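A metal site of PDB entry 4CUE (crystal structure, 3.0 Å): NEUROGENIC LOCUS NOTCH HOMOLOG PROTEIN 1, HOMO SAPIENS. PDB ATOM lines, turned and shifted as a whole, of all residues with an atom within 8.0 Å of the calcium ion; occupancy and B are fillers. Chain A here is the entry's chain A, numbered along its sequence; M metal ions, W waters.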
ATOM      1  N   PRO A  72       0.360  14.841 -20.234  1.00  0.00           N
ATOM      2  CA  PRO A  72       0.664  16.110 -20.914  1.00  0.00           C
ATOM      3  C   PRO A  72      -0.555  16.658 -21.656  1.00  0.00           C
ATOM      4  O   PRO A  72      -1.323  15.888 -22.251  1.00  0.00           O
ATOM      5  CB  PRO A  72       1.795  15.762 -21.872  1.00  0.00           C
ATOM      6  CG  PRO A  72       2.320  14.476 -21.393  1.00  0.00           C
ATOM      7  CD  PRO A  72       1.199  13.745 -20.745  1.00  0.00           C
ATOM      8  N   GLY A  73      -0.750  17.966 -21.516  1.00  0.00           N
ATOM      9  CA  GLY A  73      -1.871  18.677 -22.111  1.00  0.00           C
ATOM     10  C   GLY A  73      -3.031  18.896 -21.174  1.00  0.00           C
ATOM     11  O   GLY A  73      -3.990  19.571 -21.547  1.00  0.00           O
ATOM     12  N   TYR A  74      -2.955  18.322 -19.959  1.00  0.00           N
ATOM     13  CA  TYR A  74      -4.021  18.426 -18.957  1.00  0.00           C
ATOM     14  C   TYR A  74      -3.528  19.060 -17.716  1.00  0.00           C
ATOM     15  O   TYR A  74      -2.341  18.953 -17.393  1.00  0.00           O
ATOM     16  CB  TYR A  74      -4.619  17.062 -18.610  1.00  0.00           C
ATOM     17  CG  TYR A  74      -5.319  16.439 -19.773  1.00  0.00           C
ATOM     18  CD1 TYR A  74      -6.648  16.740 -20.055  1.00  0.00           C
ATOM     19  CD2 TYR A  74      -4.660  15.573 -20.639  1.00  0.00           C
ATOM     20  CE1 TYR A  74      -7.303  16.184 -21.148  1.00  0.00           C
ATOM     21  CE2 TYR A  74      -5.293  15.021 -21.749  1.00  0.00           C
ATOM     22  CZ  TYR A  74      -6.627  15.302 -21.985  1.00  0.00           C
ATOM     23  OH  TYR A  74      -7.314  14.739 -23.051  1.00  0.00           O
ATOM     24  N   VAL A  81      -8.939  19.793 -16.797  1.00  0.00           N
ATOM     25  CA  VAL A  81      -8.736  20.897 -17.708  1.00  0.00           C
ATOM     26  C   VAL A  81      -7.780  20.538 -18.858  1.00  0.00           C
ATOM     27  O   VAL A  81      -6.586  20.268 -18.632  1.00  0.00           O
ATOM     28  CB  VAL A  81      -8.212  22.116 -16.931  1.00  0.00           C
ATOM     29  CG1 VAL A  81      -7.866  23.271 -17.880  1.00  0.00           C
ATOM     30  CG2 VAL A  81      -9.210  22.526 -15.877  1.00  0.00           C
ATOM     31  N   ASN A  82      -8.309  20.610 -20.099  1.00  0.00           N
ATOM     32  CA  ASN A  82      -7.538  20.423 -21.298  1.00  0.00           C
ATOM     33  C   ASN A  82      -6.976  21.799 -21.563  1.00  0.00           C
ATOM     34  O   ASN A  82      -7.735  22.706 -21.909  1.00  0.00           O
ATOM     35  CB  ASN A  82      -8.442  19.949 -22.404  1.00  0.00           C
ATOM     36  CG  ASN A  82      -7.792  19.735 -23.722  1.00  0.00           C
ATOM     37  OD1 ASN A  82      -6.920  20.515 -24.144  1.00  0.00           O
ATOM     38  ND2 ASN A  82      -8.251  18.698 -24.432  1.00  0.00           N
ATOM     39  N   THR A  83      -5.669  21.992 -21.338  1.00  0.00           N
ATOM     40  CA  THR A  83      -4.984  23.281 -21.529  1.00  0.00           C
ATOM     41  C   THR A  83      -5.289  23.885 -22.891  1.00  0.00           C
ATOM     42  O   THR A  83      -5.259  23.165 -23.901  1.00  0.00           O
ATOM     43  CB  THR A  83      -3.485  23.117 -21.347  1.00  0.00           C
ATOM     44  OG1 THR A  83      -3.212  22.494 -20.085  1.00  0.00           O
ATOM     45  CG2 THR A  83      -2.781  24.457 -21.392  1.00  0.00           C
ATOM     46  N   ASP A  84      -5.628  25.174 -22.953  1.00  0.00           N
ATOM     47  CA  ASP A  84      -5.897  25.786 -24.259  1.00  0.00           C
ATOM     48  C   ASP A  84      -4.594  26.259 -24.938  1.00  0.00           C
ATOM     49  O   ASP A  84      -4.102  27.344 -24.626  1.00  0.00           O
ATOM     50  CB  ASP A  84      -6.913  26.937 -24.151  1.00  0.00           C
ATOM     51  CG  ASP A  84      -7.280  27.585 -25.488  1.00  0.00           C
ATOM     52  OD1 ASP A  84      -6.995  26.984 -26.552  1.00  0.00           O
ATOM     53  OD2 ASP A  84      -7.897  28.680 -25.472  1.00  0.00           O
ATOM     54  N   GLU A  85      -4.060  25.456 -25.862  1.00  0.00           N
ATOM     55  CA  GLU A  85      -2.816  25.820 -26.561  1.00  0.00           C
ATOM     56  C   GLU A  85      -2.978  26.958 -27.555  1.00  0.00           C
ATOM     57  O   GLU A  85      -1.997  27.563 -27.966  1.00  0.00           O
ATOM     58  CB  GLU A  85      -2.146  24.610 -27.214  1.00  0.00           C
ATOM     59  CG  GLU A  85      -1.422  23.712 -26.211  1.00  0.00           C
ATOM     60  CD  GLU A  85      -2.297  22.680 -25.526  1.00  0.00           C
ATOM     61  OE1 GLU A  85      -3.346  22.301 -26.099  1.00  0.00           O
ATOM     62  OE2 GLU A  85      -1.900  22.217 -24.424  1.00  0.00           O
ATOM     63  N   CYS A  86      -4.231  27.267 -27.911  1.00  0.00           N
ATOM     64  CA  CYS A  86      -4.579  28.319 -28.849  1.00  0.00           C
ATOM     65  C   CYS A  86      -4.587  29.676 -28.179  1.00  0.00           C
ATOM     66  O   CYS A  86      -4.673  30.679 -28.879  1.00  0.00           O
ATOM     67  CB  CYS A  86      -5.920  28.039 -29.517  1.00  0.00           C
ATOM     68  SG  CYS A  86      -5.845  26.714 -30.749  1.00  0.00           S
ATOM     69  N   LEU A  98      -7.134  25.470 -33.918  1.00  0.00           N
ATOM     70  CA  LEU A  98      -7.891  24.361 -33.343  1.00  0.00           C
ATOM     71  C   LEU A  98      -7.128  23.795 -32.171  1.00  0.00           C
ATOM     72  O   LEU A  98      -5.954  23.464 -32.320  1.00  0.00           O
ATOM     73  CB  LEU A  98      -8.171  23.287 -34.386  1.00  0.00           C
ATOM     74  CG  LEU A  98      -8.957  22.034 -33.948  1.00  0.00           C
ATOM     75  CD1 LEU A  98     -10.324  22.344 -33.296  1.00  0.00           C
ATOM     76  CD2 LEU A  98      -9.114  21.117 -35.140  1.00  0.00           C
ATOM     77  N   ASP A  99      -7.757  23.675 -31.007  1.00  0.00           N
ATOM     78  CA  ASP A  99      -7.044  23.160 -29.838  1.00  0.00           C
ATOM     79  C   ASP A  99      -7.020  21.642 -29.874  1.00  0.00           C
ATOM     80  O   ASP A  99      -7.981  21.009 -30.311  1.00  0.00           O
ATOM     81  CB  ASP A  99      -7.611  23.705 -28.532  1.00  0.00           C
ATOM     82  CG  ASP A  99      -6.896  23.212 -27.276  1.00  0.00           C
ATOM     83  OD1 ASP A  99      -5.704  23.566 -27.097  1.00  0.00           O
ATOM     84  OD2 ASP A  99      -7.518  22.465 -26.476  1.00  0.00           O
ATOM     85  N   LYS A 100      -5.881  21.061 -29.495  1.00  0.00           N
ATOM     86  CA  LYS A 100      -5.673  19.627 -29.435  1.00  0.00           C
ATOM     87  C   LYS A 100      -5.116  19.262 -28.072  1.00  0.00           C
ATOM     88  O   LYS A 100      -5.159  20.070 -27.136  1.00  0.00           O
ATOM     89  CB  LYS A 100      -4.730  19.157 -30.549  1.00  0.00           C
ATOM     90  CG  LYS A 100      -5.185  19.487 -31.933  1.00  0.00           C
ATOM     91  CD  LYS A 100      -6.464  18.752 -32.296  1.00  0.00           C
ATOM     92  CE  LYS A 100      -6.805  18.953 -33.739  1.00  0.00           C
ATOM     93  NZ  LYS A 100      -7.950  18.085 -34.141  1.00  0.00           N
ATOM     94  N   ILE A 101      -4.601  18.034 -27.951  1.00  0.00           N
ATOM     95  CA  ILE A 101      -4.014  17.583 -26.706  1.00  0.00           C
ATOM     96  C   ILE A 101      -2.525  17.915 -26.733  1.00  0.00           C
ATOM     97  O   ILE A 101      -1.780  17.341 -27.527  1.00  0.00           O
ATOM     98  CB  ILE A 101      -4.316  16.108 -26.441  1.00  0.00           C
ATOM     99  CG1 ILE A 101      -5.845  15.841 -26.527  1.00  0.00           C
ATOM    100  CG2 ILE A 101      -3.759  15.743 -25.078  1.00  0.00           C
ATOM    101  CD1 ILE A 101      -6.261  14.383 -26.812  1.00  0.00           C
ATOM    102  N   ASN A 102      -2.099  18.847 -25.875  1.00  0.00           N
ATOM    103  CA  ASN A 102      -0.722  19.330 -25.755  1.00  0.00           C
ATOM    104  C   ASN A 102      -0.196  19.808 -27.105  1.00  0.00           C
ATOM    105  O   ASN A 102       1.010  19.769 -27.371  1.00  0.00           O
ATOM    106  CB  ASN A 102       0.202  18.278 -25.108  1.00  0.00           C
ATOM    107  CG  ASN A 102       1.496  18.835 -24.588  1.00  0.00           C
ATOM    108  OD1 ASN A 102       1.593  20.004 -24.218  1.00  0.00           O
ATOM    109  ND2 ASN A 102       2.535  18.026 -24.577  1.00  0.00           N
ATOM    110  N   GLU A 103      -1.116  20.321 -27.953  1.00  0.00           N
ATOM    111  CA  GLU A 103      -0.821  20.745 -29.303  1.00  0.00           C
ATOM    112  C   GLU A 103      -1.955  21.618 -29.843  1.00  0.00           C
ATOM    113  O   GLU A 103      -3.009  21.703 -29.224  1.00  0.00           O
ATOM    114  CB  GLU A 103      -0.687  19.449 -30.154  1.00  0.00           C
ATOM    115  CG  GLU A 103      -0.236  19.617 -31.590  1.00  0.00           C
ATOM    116  CD  GLU A 103       1.066  20.377 -31.754  1.00  0.00           C
ATOM    117  OE1 GLU A 103       1.051  21.636 -31.847  1.00  0.00           O
ATOM    118  OE2 GLU A 103       2.109  19.690 -31.787  1.00  0.00           O
ATOM    119  N   PHE A 104      -1.754  22.227 -31.017  1.00  0.00           N
ATOM    120  CA  PHE A 104      -2.764  22.977 -31.738  1.00  0.00           C
ATOM    121  C   PHE A 104      -2.601  22.724 -33.229  1.00  0.00           C
ATOM    122  O   PHE A 104      -1.522  22.324 -33.679  1.00  0.00           O
ATOM    123  CB  PHE A 104      -2.659  24.481 -31.447  1.00  0.00           C
ATOM    124  CG  PHE A 104      -1.372  25.101 -31.911  1.00  0.00           C
ATOM    125  CD1 PHE A 104      -1.231  25.586 -33.220  1.00  0.00           C
ATOM    126  CD2 PHE A 104      -0.279  25.182 -31.051  1.00  0.00           C
ATOM    127  CE1 PHE A 104      -0.028  26.137 -33.655  1.00  0.00           C
ATOM    128  CE2 PHE A 104       0.913  25.740 -31.474  1.00  0.00           C
ATOM    129  CZ  PHE A 104       1.033  26.221 -32.766  1.00  0.00           C
HETATM  130 CA    CA M   1      -5.481  21.615 -25.568  1.00  0.00          CA
HETATM  131  O   HOH W   1      -4.071  20.062 -24.528  1.00  0.00           O
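The calcium ion is bound by O of Lys 100, O of Thr 83, OD1 of Asn 82, OE1 of Glu 85, water W1, OD2 of Asp 99 and OD1 of Asp 99.
Water W1 lies within hydrogen-bond range of N of Asn 102 (2.7 Å), O of Gly 73 (3.0 Å) and OE2 of Glu 85 (3.1 Å).
The backbone NH of Asp 99 lies within hydrogen-bond range of the side-chain sulfur of Cys 86. The backbone NH (N) of Thr 83 is in hydrogen-bond range of the backbone carbonyl oxygen (O) of Gly 73 (3.0 Å).
Five residues have an atom within 4 Å of the calcium ion: Asn 82, Thr 83, Glu 85, Asp 99 and Lys 100. The nearest printed residue that does not touch the calcium ion is Asn 102 (4.4 Å).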
